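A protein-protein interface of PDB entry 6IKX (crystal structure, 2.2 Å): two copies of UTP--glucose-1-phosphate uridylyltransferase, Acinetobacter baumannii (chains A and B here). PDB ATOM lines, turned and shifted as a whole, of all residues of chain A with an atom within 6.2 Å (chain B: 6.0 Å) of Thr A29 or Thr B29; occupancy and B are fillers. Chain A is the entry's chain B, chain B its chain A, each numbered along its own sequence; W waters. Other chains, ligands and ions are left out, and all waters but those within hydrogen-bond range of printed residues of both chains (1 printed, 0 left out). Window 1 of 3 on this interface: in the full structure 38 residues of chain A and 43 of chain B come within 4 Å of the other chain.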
ATOM      1  N   PHE A  16     -12.553  26.733  18.663  1.00  0.00           N
ATOM      2  CA  PHE A  16     -12.799  25.675  19.647  1.00  0.00           C
ATOM      3  C   PHE A  16     -13.626  24.693  18.848  1.00  0.00           C
ATOM      4  O   PHE A  16     -14.694  24.313  19.221  1.00  0.00           O
ATOM      5  CB  PHE A  16     -13.586  26.225  20.825  1.00  0.00           C
ATOM      6  CG  PHE A  16     -13.530  25.364  22.047  1.00  0.00           C
ATOM      7  CD1 PHE A  16     -12.330  24.985  22.581  1.00  0.00           C
ATOM      8  CD2 PHE A  16     -14.681  24.937  22.651  1.00  0.00           C
ATOM      9  CE1 PHE A  16     -12.273  24.192  23.693  1.00  0.00           C
ATOM     10  CE2 PHE A  16     -14.634  24.147  23.762  1.00  0.00           C
ATOM     11  CZ  PHE A  16     -13.425  23.779  24.288  1.00  0.00           C
ATOM     12  N   ALA A  19     -15.442  20.762  19.631  1.00  0.00           N
ATOM     13  CA  ALA A  19     -16.536  21.021  20.525  1.00  0.00           C
ATOM     14  C   ALA A  19     -17.697  21.797  19.937  1.00  0.00           C
ATOM     15  O   ALA A  19     -18.809  21.521  20.249  1.00  0.00           O
ATOM     16  CB  ALA A  19     -16.028  21.696  21.766  1.00  0.00           C
ATOM     17  N   ILE A  23     -22.852  22.135  17.813  1.00  0.00           N
ATOM     18  CA  ILE A  23     -23.499  23.112  18.739  1.00  0.00           C
ATOM     19  C   ILE A  23     -22.797  24.461  18.595  1.00  0.00           C
ATOM     20  O   ILE A  23     -21.616  24.542  18.236  1.00  0.00           O
ATOM     21  CB  ILE A  23     -23.433  22.590  20.200  1.00  0.00           C
ATOM     22  CG1 ILE A  23     -22.000  22.587  20.740  1.00  0.00           C
ATOM     23  CG2 ILE A  23     -24.080  21.209  20.330  1.00  0.00           C
ATOM     24  CD1 ILE A  23     -21.907  22.157  22.160  1.00  0.00           C
ATOM     25  N   MET A  27     -22.715  27.818  23.391  1.00  0.00           N
ATOM     26  CA  MET A  27     -23.497  26.820  24.172  1.00  0.00           C
ATOM     27  C   MET A  27     -22.533  25.788  24.785  1.00  0.00           C
ATOM     28  O   MET A  27     -22.962  24.784  25.434  1.00  0.00           O
ATOM     29  CB  MET A  27     -24.541  26.150  23.280  1.00  0.00           C
ATOM     30  CG  MET A  27     -25.643  27.092  22.879  1.00  0.00           C
ATOM     31  SD  MET A  27     -26.379  27.883  24.357  1.00  0.00           S
ATOM     32  CE  MET A  27     -26.998  26.379  25.120  1.00  0.00           C
ATOM     33  N   VAL A  28     -21.252  26.084  24.696  1.00  0.00           N
ATOM     34  CA  VAL A  28     -20.211  25.193  25.275  1.00  0.00           C
ATOM     35  C   VAL A  28     -20.317  25.248  26.809  1.00  0.00           C
ATOM     36  O   VAL A  28     -20.530  26.346  27.384  1.00  0.00           O
ATOM     37  CB  VAL A  28     -18.830  25.540  24.695  1.00  0.00           C
ATOM     38  CG1 VAL A  28     -17.713  25.462  25.701  1.00  0.00           C
ATOM     39  CG2 VAL A  28     -18.549  24.677  23.465  1.00  0.00           C
ATOM     40  N   THR A  29     -20.169  24.072  27.418  1.00  0.00           N
ATOM     41  CA  THR A  29     -20.432  23.769  28.830  1.00  0.00           C
ATOM     42  C   THR A  29     -19.267  24.277  29.679  1.00  0.00           C
ATOM     43  O   THR A  29     -18.137  23.846  29.425  1.00  0.00           O
ATOM     44  CB  THR A  29     -20.784  22.283  28.962  1.00  0.00           C
ATOM     45  OG1 THR A  29     -21.966  22.085  28.180  1.00  0.00           O
ATOM     46  CG2 THR A  29     -21.041  21.912  30.402  1.00  0.00           C
ATOM     47  N   VAL A  30     -19.574  25.163  30.640  1.00  0.00           N
ATOM     48  CA  VAL A  30     -18.619  25.798  31.593  1.00  0.00           C
ATOM     49  C   VAL A  30     -19.095  25.407  33.007  1.00  0.00           C
ATOM     50  O   VAL A  30     -20.032  26.054  33.533  1.00  0.00           O
ATOM     51  CB  VAL A  30     -18.549  27.325  31.364  1.00  0.00           C
ATOM     52  CG1 VAL A  30     -17.530  28.013  32.265  1.00  0.00           C
ATOM     53  CG2 VAL A  30     -18.234  27.681  29.921  1.00  0.00           C
ATOM     54  N   VAL A  31     -18.551  24.310  33.547  1.00  0.00           N
ATOM     55  CA  VAL A  31     -18.971  23.639  34.814  1.00  0.00           C
ATOM     56  C   VAL A  31     -20.320  22.931  34.660  1.00  0.00           C
ATOM     57  O   VAL A  31     -20.311  21.693  34.813  1.00  0.00           O
ATOM     58  CB  VAL A  31     -19.002  24.613  36.000  1.00  0.00           C
ATOM     59  CG1 VAL A  31     -19.046  23.854  37.320  1.00  0.00           C
ATOM     60  CG2 VAL A  31     -17.798  25.543  35.962  1.00  0.00           C
ATOM     61  N   ASP A  32     -21.433  23.666  34.466  1.00  0.00           N
ATOM     62  CA  ASP A  32     -22.807  23.089  34.432  1.00  0.00           C
ATOM     63  C   ASP A  32     -23.762  23.886  33.545  1.00  0.00           C
ATOM     64  O   ASP A  32     -24.958  23.560  33.515  1.00  0.00           O
ATOM     65  CB  ASP A  32     -23.393  23.040  35.839  1.00  0.00           C
ATOM     66  CG  ASP A  32     -23.521  24.403  36.527  1.00  0.00           C
ATOM     67  OD1 ASP A  32     -22.979  25.405  36.013  1.00  0.00           O
ATOM     68  OD2 ASP A  32     -24.144  24.461  37.593  1.00  0.00           O
ATOM     69  N   ARG A  33     -23.293  24.908  32.842  1.00  0.00           N
ATOM     70  CA  ARG A  33     -24.177  25.811  32.053  1.00  0.00           C
ATOM     71  C   ARG A  33     -23.397  26.270  30.819  1.00  0.00           C
ATOM     72  O   ARG A  33     -22.157  26.248  30.803  1.00  0.00           O
ATOM     73  CB  ARG A  33     -24.698  26.951  32.953  1.00  0.00           C
ATOM     74  CG  ARG A  33     -23.608  27.768  33.634  1.00  0.00           C
ATOM     75  CD  ARG A  33     -24.025  28.578  34.867  1.00  0.00           C
ATOM     76  NE  ARG A  33     -24.434  27.754  36.011  1.00  0.00           N
ATOM     77  CZ  ARG A  33     -25.690  27.597  36.429  1.00  0.00           C
ATOM     78  NH1 ARG A  33     -26.684  28.231  35.849  1.00  0.00           N
ATOM     79  NH2 ARG A  33     -25.964  26.797  37.435  1.00  0.00           N
ATOM     80  N   PRO A  34     -24.097  26.690  29.742  1.00  0.00           N
ATOM     81  CA  PRO A  34     -23.419  27.210  28.566  1.00  0.00           C
ATOM     82  C   PRO A  34     -22.685  28.514  28.922  1.00  0.00           C
ATOM     83  O   PRO A  34     -23.199  29.223  29.764  1.00  0.00           O
ATOM     84  CB  PRO A  34     -24.549  27.450  27.561  1.00  0.00           C
ATOM     85  CG  PRO A  34     -25.767  27.657  28.439  1.00  0.00           C
ATOM     86  CD  PRO A  34     -25.557  26.700  29.591  1.00  0.00           C
ATOM     87  N   ALA A  35     -21.542  28.782  28.263  1.00  0.00           N
ATOM     88  CA  ALA A  35     -20.718  30.009  28.364  1.00  0.00           C
ATOM     89  C   ALA A  35     -21.588  31.271  28.249  1.00  0.00           C
ATOM     90  O   ALA A  35     -21.386  32.240  29.026  1.00  0.00           O
ATOM     91  CB  ALA A  35     -19.653  29.978  27.290  1.00  0.00           C
ATOM     92  N   TYR A 264     -10.574  28.325  27.829  1.00  0.00           N
ATOM     93  CA  TYR A 264     -11.823  27.606  28.201  1.00  0.00           C
ATOM     94  C   TYR A 264     -11.557  26.689  29.415  1.00  0.00           C
ATOM     95  O   TYR A 264     -12.324  26.713  30.388  1.00  0.00           O
ATOM     96  CB  TYR A 264     -12.396  26.876  26.994  1.00  0.00           C
ATOM     97  CG  TYR A 264     -13.326  25.758  27.365  1.00  0.00           C
ATOM     98  CD1 TYR A 264     -14.666  25.999  27.607  1.00  0.00           C
ATOM     99  CD2 TYR A 264     -12.841  24.484  27.563  1.00  0.00           C
ATOM    100  CE1 TYR A 264     -15.524  24.984  27.983  1.00  0.00           C
ATOM    101  CE2 TYR A 264     -13.691  23.447  27.900  1.00  0.00           C
ATOM    102  CZ  TYR A 264     -15.035  23.702  28.103  1.00  0.00           C
ATOM    103  OH  TYR A 264     -15.848  22.691  28.471  1.00  0.00           O
ATOM    104  N   VAL A 268     -13.155  26.701  33.286  1.00  0.00           N
ATOM    105  CA  VAL A 268     -13.784  25.523  33.960  1.00  0.00           C
ATOM    106  C   VAL A 268     -13.187  25.399  35.363  1.00  0.00           C
ATOM    107  O   VAL A 268     -13.958  25.346  36.295  1.00  0.00           O
ATOM    108  CB  VAL A 268     -13.661  24.221  33.154  1.00  0.00           C
ATOM    109  CG2 VAL A 268     -14.467  24.313  31.856  1.00  0.00           C
ATOM    110  N   PHE B  16     -27.798  16.924  35.081  1.00  0.00           N
ATOM    111  CA  PHE B  16     -26.905  17.895  34.381  1.00  0.00           C
ATOM    112  C   PHE B  16     -27.821  18.890  33.700  1.00  0.00           C
ATOM    113  O   PHE B  16     -27.660  19.182  32.554  1.00  0.00           O
ATOM    114  CB  PHE B  16     -25.922  17.233  33.384  1.00  0.00           C
ATOM    115  CG  PHE B  16     -24.592  17.868  33.301  1.00  0.00           C
ATOM    116  CD1 PHE B  16     -24.333  19.058  33.910  1.00  0.00           C
ATOM    117  CD2 PHE B  16     -23.597  17.254  32.595  1.00  0.00           C
ATOM    118  CE1 PHE B  16     -23.097  19.625  33.823  1.00  0.00           C
ATOM    119  CE2 PHE B  16     -22.363  17.816  32.499  1.00  0.00           C
ATOM    120  CZ  PHE B  16     -22.112  19.004  33.118  1.00  0.00           C
ATOM    121  N   ALA B  19     -27.047  22.779  31.738  1.00  0.00           N
ATOM    122  CA  ALA B  19     -26.186  22.461  30.561  1.00  0.00           C
ATOM    123  C   ALA B  19     -26.960  21.741  29.453  1.00  0.00           C
ATOM    124  O   ALA B  19     -26.688  22.059  28.313  1.00  0.00           O
ATOM    125  CB  ALA B  19     -24.990  21.636  30.949  1.00  0.00           C
ATOM    126  N   ILE B  23     -29.188  21.804  24.704  1.00  0.00           N
ATOM    127  CA  ILE B  23     -28.373  20.905  23.845  1.00  0.00           C
ATOM    128  C   ILE B  23     -28.463  19.508  24.429  1.00  0.00           C
ATOM    129  O   ILE B  23     -28.585  19.321  25.624  1.00  0.00           O
ATOM    130  CB  ILE B  23     -26.880  21.330  23.741  1.00  0.00           C
ATOM    131  CG1 ILE B  23     -26.168  21.236  25.093  1.00  0.00           C
ATOM    132  CG2 ILE B  23     -26.734  22.696  23.098  1.00  0.00           C
ATOM    133  CD1 ILE B  23     -24.685  21.519  25.056  1.00  0.00           C
ATOM    134  N   MET B  27     -23.935  15.972  24.031  1.00  0.00           N
ATOM    135  CA  MET B  27     -23.169  17.026  23.301  1.00  0.00           C
ATOM    136  C   MET B  27     -22.435  17.947  24.281  1.00  0.00           C
ATOM    137  O   MET B  27     -21.803  18.939  23.862  1.00  0.00           O
ATOM    138  CB  MET B  27     -24.080  17.823  22.360  1.00  0.00           C
ATOM    139  CG  MET B  27     -24.506  16.997  21.156  1.00  0.00           C
ATOM    140  SD  MET B  27     -23.072  16.210  20.343  1.00  0.00           S
ATOM    141  CE  MET B  27     -22.515  17.664  19.466  1.00  0.00           C
ATOM    142  N   VAL B  28     -22.430  17.571  25.542  1.00  0.00           N
ATOM    143  CA  VAL B  28     -21.742  18.316  26.623  1.00  0.00           C
ATOM    144  C   VAL B  28     -20.225  18.132  26.495  1.00  0.00           C
ATOM    145  O   VAL B  28     -19.735  16.975  26.400  1.00  0.00           O
ATOM    146  CB  VAL B  28     -22.314  17.809  27.953  1.00  0.00           C
ATOM    147  CG1 VAL B  28     -21.344  17.886  29.110  1.00  0.00           C
ATOM    148  CG2 VAL B  28     -23.606  18.561  28.247  1.00  0.00           C
ATOM    149  N   THR B  29     -19.487  19.228  26.588  1.00  0.00           N
ATOM    150  CA  THR B  29     -18.084  19.248  26.138  1.00  0.00           C
ATOM    151  C   THR B  29     -17.237  18.693  27.271  1.00  0.00           C
ATOM    152  O   THR B  29     -17.424  19.064  28.416  1.00  0.00           O
ATOM    153  CB  THR B  29     -17.667  20.561  25.447  1.00  0.00           C
ATOM    154  OG1 THR B  29     -16.376  20.946  25.933  1.00  0.00           O
ATOM    155  CG2 THR B  29     -18.691  21.670  25.568  1.00  0.00           C
ATOM    156  N   VAL B  30     -16.356  17.766  26.919  1.00  0.00           N
ATOM    157  CA  VAL B  30     -15.452  17.096  27.879  1.00  0.00           C
ATOM    158  C   VAL B  30     -14.040  17.367  27.389  1.00  0.00           C
ATOM    159  O   VAL B  30     -13.593  16.679  26.457  1.00  0.00           O
ATOM    160  CB  VAL B  30     -15.789  15.607  27.956  1.00  0.00           C
ATOM    161  CG1 VAL B  30     -14.749  14.826  28.757  1.00  0.00           C
ATOM    162  CG2 VAL B  30     -17.193  15.431  28.510  1.00  0.00           C
ATOM    163  N   VAL B  31     -13.426  18.408  27.944  1.00  0.00           N
ATOM    164  CA  VAL B  31     -12.128  18.971  27.486  1.00  0.00           C
ATOM    165  C   VAL B  31     -12.378  19.793  26.216  1.00  0.00           C
ATOM    166  O   VAL B  31     -12.461  21.027  26.300  1.00  0.00           O
ATOM    167  CB  VAL B  31     -11.067  17.880  27.251  1.00  0.00           C
ATOM    168  CG1 VAL B  31      -9.681  18.478  27.130  1.00  0.00           C
ATOM    169  CG2 VAL B  31     -11.095  16.822  28.335  1.00  0.00           C
ATOM    170  N   ASP B  32     -12.451  19.150  25.061  1.00  0.00           N
ATOM    171  CA  ASP B  32     -12.554  19.889  23.788  1.00  0.00           C
ATOM    172  C   ASP B  32     -13.451  19.174  22.776  1.00  0.00           C
ATOM    173  O   ASP B  32     -13.406  19.603  21.595  1.00  0.00           O
ATOM    174  CB  ASP B  32     -11.142  20.042  23.228  1.00  0.00           C
ATOM    175  CG  ASP B  32     -10.506  18.730  22.773  1.00  0.00           C
ATOM    176  OD1 ASP B  32     -11.034  17.667  23.129  1.00  0.00           O
ATOM    177  OD2 ASP B  32      -9.486  18.795  22.044  1.00  0.00           O
ATOM    178  N   ARG B  33     -14.194  18.122  23.161  1.00  0.00           N
ATOM    179  CA  ARG B  33     -15.169  17.460  22.246  1.00  0.00           C
ATOM    180  C   ARG B  33     -16.405  16.957  23.006  1.00  0.00           C
ATOM    181  O   ARG B  33     -16.383  16.745  24.203  1.00  0.00           O
ATOM    182  CB  ARG B  33     -14.430  16.329  21.532  1.00  0.00           C
ATOM    183  CG  ARG B  33     -14.020  15.215  22.469  1.00  0.00           C
ATOM    184  CD  ARG B  33     -12.807  14.428  22.033  1.00  0.00           C
ATOM    185  NE  ARG B  33     -11.642  15.280  21.862  1.00  0.00           N
ATOM    186  CZ  ARG B  33     -10.984  15.468  20.726  1.00  0.00           C
ATOM    187  NH1 ARG B  33     -11.340  14.841  19.619  1.00  0.00           N
ATOM    188  NH2 ARG B  33      -9.964  16.294  20.707  1.00  0.00           N
ATOM    189  N   PRO B  34     -17.564  16.740  22.367  1.00  0.00           N
ATOM    190  CA  PRO B  34     -18.733  16.253  23.103  1.00  0.00           C
ATOM    191  C   PRO B  34     -18.516  14.831  23.676  1.00  0.00           C
ATOM    192  O   PRO B  34     -17.740  14.035  23.126  1.00  0.00           O
ATOM    193  CB  PRO B  34     -19.816  16.323  22.005  1.00  0.00           C
ATOM    194  CG  PRO B  34     -19.034  16.001  20.757  1.00  0.00           C
ATOM    195  CD  PRO B  34     -17.817  16.884  20.933  1.00  0.00           C
ATOM    196  N   ALA B  35     -19.179  14.543  24.797  1.00  0.00           N
ATOM    197  CA  ALA B  35     -19.051  13.287  25.576  1.00  0.00           C
ATOM    198  C   ALA B  35     -19.246  12.083  24.631  1.00  0.00           C
ATOM    199  O   ALA B  35     -18.518  11.094  24.757  1.00  0.00           O
ATOM    200  CB  ALA B  35     -20.056  13.315  26.716  1.00  0.00           C
ATOM    201  N   TYR B 264     -19.017  14.327  35.812  1.00  0.00           N
ATOM    202  CA  TYR B 264     -18.630  15.174  34.653  1.00  0.00           C
ATOM    203  C   TYR B 264     -17.316  15.915  34.957  1.00  0.00           C
ATOM    204  O   TYR B 264     -16.306  15.667  34.250  1.00  0.00           O
ATOM    205  CB  TYR B 264     -19.765  16.118  34.266  1.00  0.00           C
ATOM    206  CG  TYR B 264     -19.375  17.181  33.272  1.00  0.00           C
ATOM    207  CD1 TYR B 264     -19.147  16.864  31.939  1.00  0.00           C
ATOM    208  CD2 TYR B 264     -19.194  18.502  33.683  1.00  0.00           C
ATOM    209  CE1 TYR B 264     -18.739  17.836  31.037  1.00  0.00           C
ATOM    210  CE2 TYR B 264     -18.854  19.489  32.777  1.00  0.00           C
ATOM    211  CZ  TYR B 264     -18.599  19.146  31.465  1.00  0.00           C
ATOM    212  OH  TYR B 264     -18.236  20.120  30.606  1.00  0.00           O
ATOM    213  N   VAL B 268     -13.641  15.601  33.064  1.00  0.00           N
ATOM    214  CA  VAL B 268     -12.919  16.754  32.464  1.00  0.00           C
ATOM    215  C   VAL B 268     -11.503  16.759  33.032  1.00  0.00           C
ATOM    216  O   VAL B 268     -10.586  17.020  32.286  1.00  0.00           O
ATOM    217  CB  VAL B 268     -13.634  18.087  32.711  1.00  0.00           C
ATOM    218  CG1 VAL B 268     -12.773  19.259  32.247  1.00  0.00           C
ATOM    219  CG2 VAL B 268     -15.005  18.107  32.048  1.00  0.00           C
HETATM  220  O   HOH W   1     -19.207  19.654  22.911  1.00  0.00           O
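Water W1 bridges O of Met B27 (2.9 Å) and O of Ala A19 (3.3 Å).
Ile A23 touches Met B27, and with the chains exchanged Met A27 touches Ile B23.
Thr A29 touches its own counterpart, Thr B29.
Val A31 touches Tyr B264, and with the chains exchanged Tyr A264 touches Val B31.
Asp A32 touches Phe B16, but with the chains exchanged Phe A16 does not touch Asp B32 (4.02 Å).
Of the 15 pairs that touch across the chains among the printed residues, 13 have their exchanged pair printed and touching as well.
Among the printed residues, merely in contact across the chains: Tyr A264 with Val B31, Thr A29 with Tyr B264, Val A31 with Tyr B264, Thr A29 with Thr B29, Asp A32 with Phe B16, Phe A16 with Val B31, Val A31 with Phe B16, Ile A23 with Met B27, Val A28 with Thr B29, Met A27 with Ile B23, Thr A29 with Val B28 and Thr A29 with Ala B19.
The backbone NH of Ala A19 lies within hydrogen-bond range of the backbone carbonyl oxygen of Asp B32 (3.1 Å).
The backbone carbonyl oxygen of Asp A32 is in hydrogen-bond range of the backbone NH of Ala B19 (2.9 Å).
OG1 of Thr B29 sits at hydrogen-bond distance from OH of Tyr A264 (3.1 Å).
Printed residues of chain B within 4 Å of Thr A29: Ala B19 (3.996 Å), Val B28 (3.9 Å), Thr B29 (3.4 Å) and Tyr B264 (3.3 Å).
Thr B29 touches just these residues of chain A: Val A28, Thr A29 and Tyr A264.
Of the printed residues of chain A, Val B31 touches Phe A16 (3.5 Å) and Tyr A264 (3.2 Å).
Printed residues of chain B within 4 Å of Ile A23: Met B27 (3.6 Å).
Of the printed residues of chain A, Val B28 touches Thr A29 (3.9 Å).
Of the printed residues of chain B, Tyr A264 touches Thr B29 and Val B31.
Val B268 touches none of the printed residues of chain A.
The nearest residue of chain A that does not touch Thr B29 is Ala A19 (4.2 Å).
Of the 14 printed residues of chain B, 9 touch a printed residue of chain A.
Hydrophobic or aromatic side chains of chain B within 4 Å of the printed part of chain A: Phe B16, Ala B19, Ile B23, Met B27, Val B28 and Tyr B264.
Printed residues of chain A that touch a printed residue of chain B: Phe A16, Ala A19, Ile A23, Met A27, Val A28, Thr A29, Val A31, Asp A32 and Tyr A264.
Hydrophobic or aromatic side chains of chain A within 4 Å of the printed part of chain B: Phe A16, Ala A19, Ile A23, Val A28 and Tyr A264.
Among the printed residues, 15 pairs touch across the chains.
NE of Arg A33 lies within salt-bridge range of OD1 of Asp A32, at 2.8 Å.
The backbone carbonyl oxygen of Thr B29 lies within hydrogen-bond range of the side-chain hydroxyl of Tyr B264, at 2.6 Å.
O of Thr A29 is in hydrogen-bond range of OH of Tyr A264, at 2.7 Å.
NE of Arg B33 is in salt-bridge range of OD1 of Asp B32 (2.8 Å).
O of Val A28 sits at hydrogen-bond distance from N of Ala A35 (2.8 Å).
The backbone carbonyl oxygen (O) of Val B28 sits at hydrogen-bond distance from the backbone NH (N) of Ala B35.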
